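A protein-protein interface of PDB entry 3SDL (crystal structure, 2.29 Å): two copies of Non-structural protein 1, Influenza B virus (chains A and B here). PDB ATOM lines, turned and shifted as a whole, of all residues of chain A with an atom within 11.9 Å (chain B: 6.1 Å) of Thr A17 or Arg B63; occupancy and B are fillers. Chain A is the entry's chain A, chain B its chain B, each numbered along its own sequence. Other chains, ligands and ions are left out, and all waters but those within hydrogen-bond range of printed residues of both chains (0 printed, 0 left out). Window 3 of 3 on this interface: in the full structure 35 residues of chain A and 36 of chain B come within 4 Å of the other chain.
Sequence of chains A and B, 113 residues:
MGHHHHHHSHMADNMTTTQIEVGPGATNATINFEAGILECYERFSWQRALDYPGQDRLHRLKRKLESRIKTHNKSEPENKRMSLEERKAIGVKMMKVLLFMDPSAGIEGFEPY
NH2 of Arg A57 lies close to NH1 of Arg B68, at 3.3 Å.
NE of Arg B63 sits close to O of His B59.
The side-chain hydroxyl (OG) of Ser B67 is in hydrogen-bond range of the backbone carbonyl oxygen (O) of Lys B64 (2.6 Å).
The backbone carbonyl oxygen (O) of Arg B63 sits at hydrogen-bond distance from the side-chain hydroxyl (OG) of Ser B67 (3.4 Å).
Among the printed residues, pairs that only touch across the chains: Thr A17 with Arg B63, Thr A17 with His B59, Arg A57 with Lys B64 and Thr A18 with His B59.
Thr A17 touches just these residues of chain B: His B59 (3.6 Å) and Arg B63 (3.3 Å).
Arg B63 touches just one residue of chain A: Thr A17.
No residue of chain A comes within 4 Å of Asp B56.
Of chain A, only Thr A17 (3.6 Å) and Thr A18 (3.7 Å) come within 4 Å of His B59.
No residue of chain A comes within 4 Å of Arg B60.
No residue of chain A comes within 4 Å of Leu B61.
No residue of chain A comes within 4 Å of Lys B62.
No residue of chain A comes within 4 Å of Glu B66.
Ser B67 touches none of the printed residues of chain A.
Printed residues of chain B within 4 Å of Arg A57: Lys B64 (3.7 Å) and Arg B68 (3.3 Å).
Of the printed residues of chain B, Thr A18 touches His B59 (3.7 Å).
Printed residues of chain A within 4 Å of Arg B68: Arg A57 (3.3 Å).
Glu A21 touches none of the printed residues of chain B.
Leu B58 touches none of the printed residues of chain A.
The nearest printed residue of chain B that does not touch Thr A17 is Lys B62 (6.1 Å).
Printed residues of chain B that touch a printed residue of chain A: His B59, Arg B63, Lys B64 and Arg B68.
Printed residues of chain A that touch a printed residue of chain B: Thr A17, Thr A18 and Arg A57.
Among the printed residues, no Asp or Glu carboxylate lies within 4 Å of a Lys or Arg side-chain nitrogen of the other chain.
No position is printed for both chains.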
ATOM      1  N   THR A  17      -7.614  28.420  -9.257  1.00  0.00           N
ATOM      2  CA  THR A  17      -7.393  27.001  -9.006  1.00  0.00           C
ATOM      3  C   THR A  17      -7.686  26.159 -10.244  1.00  0.00           C
ATOM      4  O   THR A  17      -8.548  25.282 -10.220  1.00  0.00           O
ATOM      5  CB  THR A  17      -8.254  26.491  -7.833  1.00  0.00           C
ATOM      6  OG1 THR A  17      -9.637  26.746  -8.103  1.00  0.00           O
ATOM      7  CG2 THR A  17      -7.860  27.183  -6.538  1.00  0.00           C
ATOM      8  N   THR A  18      -6.966  26.438 -11.326  1.00  0.00           N
ATOM      9  CA  THR A  18      -7.114  25.677 -12.564  1.00  0.00           C
ATOM     10  C   THR A  18      -5.776  25.097 -13.019  1.00  0.00           C
ATOM     11  O   THR A  18      -4.870  25.824 -13.423  1.00  0.00           O
ATOM     12  CB  THR A  18      -7.715  26.534 -13.691  1.00  0.00           C
ATOM     13  OG1 THR A  18      -8.996  27.031 -13.283  1.00  0.00           O
ATOM     14  CG2 THR A  18      -7.881  25.707 -14.955  1.00  0.00           C
ATOM     15  N   GLN A  19      -5.666  23.775 -12.958  1.00  0.00           N
ATOM     16  CA  GLN A  19      -4.405  23.094 -13.223  1.00  0.00           C
ATOM     17  C   GLN A  19      -4.009  23.079 -14.699  1.00  0.00           C
ATOM     18  O   GLN A  19      -4.856  22.953 -15.583  1.00  0.00           O
ATOM     19  CB  GLN A  19      -4.454  21.667 -12.673  1.00  0.00           C
ATOM     20  CG  GLN A  19      -3.193  20.873 -12.914  1.00  0.00           C
ATOM     21  CD  GLN A  19      -3.083  19.679 -11.994  1.00  0.00           C
ATOM     22  OE1 GLN A  19      -3.154  18.530 -12.431  1.00  0.00           O
ATOM     23  NE2 GLN A  19      -2.909  19.945 -10.703  1.00  0.00           N
ATOM     24  N   ILE A  20      -2.709  23.203 -14.952  1.00  0.00           N
ATOM     25  CA  ILE A  20      -2.172  23.153 -16.306  1.00  0.00           C
ATOM     26  C   ILE A  20      -1.322  21.903 -16.491  1.00  0.00           C
ATOM     27  O   ILE A  20      -0.320  21.719 -15.802  1.00  0.00           O
ATOM     28  CB  ILE A  20      -1.301  24.381 -16.606  1.00  0.00           C
ATOM     29  CG1 ILE A  20      -2.113  25.664 -16.431  1.00  0.00           C
ATOM     30  CG2 ILE A  20      -0.727  24.295 -18.009  1.00  0.00           C
ATOM     31  CD1 ILE A  20      -1.314  26.920 -16.671  1.00  0.00           C
ATOM     32  N   GLU A  21      -1.728  21.047 -17.422  1.00  0.00           N
ATOM     33  CA  GLU A  21      -1.028  19.789 -17.671  1.00  0.00           C
ATOM     34  C   GLU A  21       0.420  20.013 -18.087  1.00  0.00           C
ATOM     35  O   GLU A  21       0.708  20.860 -18.933  1.00  0.00           O
ATOM     36  CB  GLU A  21      -1.756  18.977 -18.742  1.00  0.00           C
ATOM     37  CG  GLU A  21      -1.104  17.639 -19.050  1.00  0.00           C
ATOM     38  CD  GLU A  21      -1.889  16.826 -20.067  1.00  0.00           C
ATOM     39  OE1 GLU A  21      -2.944  17.309 -20.531  1.00  0.00           O
ATOM     40  OE2 GLU A  21      -1.450  15.704 -20.401  1.00  0.00           O
ATOM     41  N   ARG A  57       8.984  31.573   5.853  1.00  0.00           N
ATOM     42  CA  ARG A  57       8.701  31.024   4.534  1.00  0.00           C
ATOM     43  C   ARG A  57       9.971  30.946   3.688  1.00  0.00           C
ATOM     44  O   ARG A  57      10.091  30.089   2.814  1.00  0.00           O
ATOM     45  CB  ARG A  57       7.621  31.844   3.822  1.00  0.00           C
ATOM     46  CG  ARG A  57       6.247  31.714   4.461  1.00  0.00           C
ATOM     47  CD  ARG A  57       5.153  32.320   3.597  1.00  0.00           C
ATOM     48  NE  ARG A  57       5.225  33.778   3.545  1.00  0.00           N
ATOM     49  CZ  ARG A  57       4.763  34.583   4.497  1.00  0.00           C
ATOM     50  NH1 ARG A  57       4.205  34.073   5.587  1.00  0.00           N
ATOM     51  NH2 ARG A  57       4.866  35.899   4.364  1.00  0.00           N
ATOM     52  N   ASP B  56       0.452  23.867  -6.794  1.00  0.00           N
ATOM     53  CA  ASP B  56      -0.234  23.843  -5.512  1.00  0.00           C
ATOM     54  C   ASP B  56       0.272  24.978  -4.626  1.00  0.00           C
ATOM     55  O   ASP B  56      -0.512  25.675  -3.983  1.00  0.00           O
ATOM     56  CB  ASP B  56      -0.035  22.493  -4.825  1.00  0.00           C
ATOM     57  CG  ASP B  56      -0.754  22.408  -3.498  1.00  0.00           C
ATOM     58  OD1 ASP B  56      -2.002  22.376  -3.501  1.00  0.00           O
ATOM     59  OD2 ASP B  56      -0.073  22.368  -2.454  1.00  0.00           O
ATOM     60  N   LEU B  58       1.561  27.644  -5.728  1.00  0.00           N
ATOM     61  CA  LEU B  58       1.074  28.849  -6.395  1.00  0.00           C
ATOM     62  C   LEU B  58      -0.290  29.252  -5.850  1.00  0.00           C
ATOM     63  O   LEU B  58      -0.483  30.384  -5.411  1.00  0.00           O
ATOM     64  CB  LEU B  58       0.981  28.627  -7.910  1.00  0.00           C
ATOM     65  CG  LEU B  58       0.585  29.816  -8.798  1.00  0.00           C
ATOM     66  CD1 LEU B  58       0.872  29.515 -10.259  1.00  0.00           C
ATOM     67  CD2 LEU B  58      -0.879  30.219  -8.616  1.00  0.00           C
ATOM     68  N   HIS B  59      -1.235  28.319  -5.889  1.00  0.00           N
ATOM     69  CA  HIS B  59      -2.607  28.598  -5.472  1.00  0.00           C
ATOM     70  C   HIS B  59      -2.738  28.824  -3.965  1.00  0.00           C
ATOM     71  O   HIS B  59      -3.590  29.594  -3.519  1.00  0.00           O
ATOM     72  CB  HIS B  59      -3.547  27.484  -5.939  1.00  0.00           C
ATOM     73  CG  HIS B  59      -3.689  27.399  -7.428  1.00  0.00           C
ATOM     74  ND1 HIS B  59      -3.664  26.201  -8.110  1.00  0.00           N
ATOM     75  CD2 HIS B  59      -3.861  28.361  -8.363  1.00  0.00           C
ATOM     76  CE1 HIS B  59      -3.812  26.430  -9.403  1.00  0.00           C
ATOM     77  NE2 HIS B  59      -3.936  27.733  -9.583  1.00  0.00           N
ATOM     78  N   ARG B  60      -1.898  28.152  -3.182  1.00  0.00           N
ATOM     79  CA  ARG B  60      -1.880  28.370  -1.741  1.00  0.00           C
ATOM     80  C   ARG B  60      -1.444  29.797  -1.449  1.00  0.00           C
ATOM     81  O   ARG B  60      -2.078  30.505  -0.668  1.00  0.00           O
ATOM     82  CB  ARG B  60      -0.933  27.389  -1.049  1.00  0.00           C
ATOM     83  CG  ARG B  60      -1.386  25.943  -1.095  1.00  0.00           C
ATOM     84  CD  ARG B  60      -0.549  25.073  -0.174  1.00  0.00           C
ATOM     85  NE  ARG B  60      -0.943  23.671  -0.251  1.00  0.00           N
ATOM     86  CZ  ARG B  60      -1.967  23.141   0.413  1.00  0.00           C
ATOM     87  NH1 ARG B  60      -2.708  23.900   1.209  1.00  0.00           N
ATOM     88  NH2 ARG B  60      -2.250  21.853   0.280  1.00  0.00           N
ATOM     89  N   LEU B  61      -0.356  30.214  -2.089  1.00  0.00           N
ATOM     90  CA  LEU B  61       0.165  31.561  -1.918  1.00  0.00           C
ATOM     91  C   LEU B  61      -0.888  32.591  -2.288  1.00  0.00           C
ATOM     92  O   LEU B  61      -1.039  33.603  -1.608  1.00  0.00           O
ATOM     93  CB  LEU B  61       1.416  31.769  -2.775  1.00  0.00           C
ATOM     94  CG  LEU B  61       1.987  33.189  -2.804  1.00  0.00           C
ATOM     95  CD1 LEU B  61       2.463  33.618  -1.422  1.00  0.00           C
ATOM     96  CD2 LEU B  61       3.114  33.289  -3.818  1.00  0.00           C
ATOM     97  N   LYS B  62      -1.617  32.333  -3.368  1.00  0.00           N
ATOM     98  CA  LYS B  62      -2.648  33.264  -3.814  1.00  0.00           C
ATOM     99  C   LYS B  62      -3.752  33.427  -2.772  1.00  0.00           C
ATOM    100  O   LYS B  62      -4.207  34.540  -2.513  1.00  0.00           O
ATOM    101  CB  LYS B  62      -3.237  32.836  -5.161  1.00  0.00           C
ATOM    102  CG  LYS B  62      -4.378  33.730  -5.629  1.00  0.00           C
ATOM    103  CD  LYS B  62      -4.727  33.488  -7.087  1.00  0.00           C
ATOM    104  CE  LYS B  62      -5.800  34.456  -7.559  1.00  0.00           C
ATOM    105  NZ  LYS B  62      -6.104  34.287  -9.008  1.00  0.00           N
ATOM    106  N   ARG B  63      -4.178  32.315  -2.177  1.00  0.00           N
ATOM    107  CA  ARG B  63      -5.202  32.353  -1.135  1.00  0.00           C
ATOM    108  C   ARG B  63      -4.704  33.119   0.087  1.00  0.00           C
ATOM    109  O   ARG B  63      -5.305  34.112   0.494  1.00  0.00           O
ATOM    110  CB  ARG B  63      -5.613  30.934  -0.732  1.00  0.00           C
ATOM    111  CG  ARG B  63      -6.187  30.114  -1.873  1.00  0.00           C
ATOM    112  CD  ARG B  63      -6.245  28.634  -1.529  1.00  0.00           C
ATOM    113  NE  ARG B  63      -6.392  27.812  -2.727  1.00  0.00           N
ATOM    114  CZ  ARG B  63      -6.298  26.487  -2.744  1.00  0.00           C
ATOM    115  NH1 ARG B  63      -6.053  25.820  -1.624  1.00  0.00           N
ATOM    116  NH2 ARG B  63      -6.443  25.826  -3.885  1.00  0.00           N
ATOM    117  N   LYS B  64      -3.602  32.646   0.664  1.00  0.00           N
ATOM    118  CA  LYS B  64      -2.990  33.289   1.821  1.00  0.00           C
ATOM    119  C   LYS B  64      -2.815  34.783   1.581  1.00  0.00           C
ATOM    120  O   LYS B  64      -3.223  35.609   2.396  1.00  0.00           O
ATOM    121  CB  LYS B  64      -1.622  32.670   2.108  1.00  0.00           C
ATOM    122  CG  LYS B  64      -1.645  31.179   2.384  1.00  0.00           C
ATOM    123  CD  LYS B  64      -0.309  30.547   2.011  1.00  0.00           C
ATOM    124  CE  LYS B  64       0.858  31.350   2.569  1.00  0.00           C
ATOM    125  NZ  LYS B  64       2.165  30.896   2.019  1.00  0.00           N
ATOM    126  N   LEU B  65      -2.202  35.115   0.451  1.00  0.00           N
ATOM    127  CA  LEU B  65      -1.910  36.498   0.095  1.00  0.00           C
ATOM    128  C   LEU B  65      -3.183  37.342   0.007  1.00  0.00           C
ATOM    129  O   LEU B  65      -3.223  38.477   0.484  1.00  0.00           O
ATOM    130  CB  LEU B  65      -1.166  36.537  -1.236  1.00  0.00           C
ATOM    131  CG  LEU B  65      -0.481  37.834  -1.654  1.00  0.00           C
ATOM    132  CD1 LEU B  65       0.569  38.229  -0.634  1.00  0.00           C
ATOM    133  CD2 LEU B  65       0.146  37.661  -3.024  1.00  0.00           C
ATOM    134  N   GLU B  66      -4.220  36.777  -0.603  1.00  0.00           N
ATOM    135  CA  GLU B  66      -5.474  37.494  -0.796  1.00  0.00           C
ATOM    136  C   GLU B  66      -6.150  37.816   0.533  1.00  0.00           C
ATOM    137  O   GLU B  66      -6.784  38.860   0.681  1.00  0.00           O
ATOM    138  CB  GLU B  66      -6.420  36.692  -1.691  1.00  0.00           C
ATOM    139  CG  GLU B  66      -7.660  37.457  -2.103  1.00  0.00           C
ATOM    140  CD  GLU B  66      -7.323  38.775  -2.768  1.00  0.00           C
ATOM    141  OE1 GLU B  66      -6.645  38.758  -3.815  1.00  0.00           O
ATOM    142  OE2 GLU B  66      -7.728  39.831  -2.238  1.00  0.00           O
ATOM    143  N   SER B  67      -6.010  36.914   1.499  1.00  0.00           N
ATOM    144  CA  SER B  67      -6.577  37.125   2.824  1.00  0.00           C
ATOM    145  C   SER B  67      -5.750  38.135   3.613  1.00  0.00           C
ATOM    146  O   SER B  67      -6.287  38.901   4.410  1.00  0.00           O
ATOM    147  CB  SER B  67      -6.675  35.802   3.588  1.00  0.00           C
ATOM    148  OG  SER B  67      -5.410  35.172   3.696  1.00  0.00           O
ATOM    149  N   ARG B  68      -4.440  38.133   3.386  1.00  0.00           N
ATOM    150  CA  ARG B  68      -3.555  39.083   4.050  1.00  0.00           C
ATOM    151  C   ARG B  68      -3.817  40.506   3.573  1.00  0.00           C
ATOM    152  O   ARG B  68      -3.739  41.453   4.353  1.00  0.00           O
ATOM    153  CB  ARG B  68      -2.088  38.714   3.823  1.00  0.00           C
ATOM    154  CG  ARG B  68      -1.563  37.622   4.743  1.00  0.00           C
ATOM    155  CD  ARG B  68      -0.038  37.613   4.744  1.00  0.00           C
ATOM    156  NE  ARG B  68       0.499  37.327   3.418  1.00  0.00           N
ATOM    157  CZ  ARG B  68       1.727  37.640   3.017  1.00  0.00           C
ATOM    158  NH1 ARG B  68       2.561  38.264   3.835  1.00  0.00           N
ATOM    159  NH2 ARG B  68       2.118  37.335   1.789  1.00  0.00           N
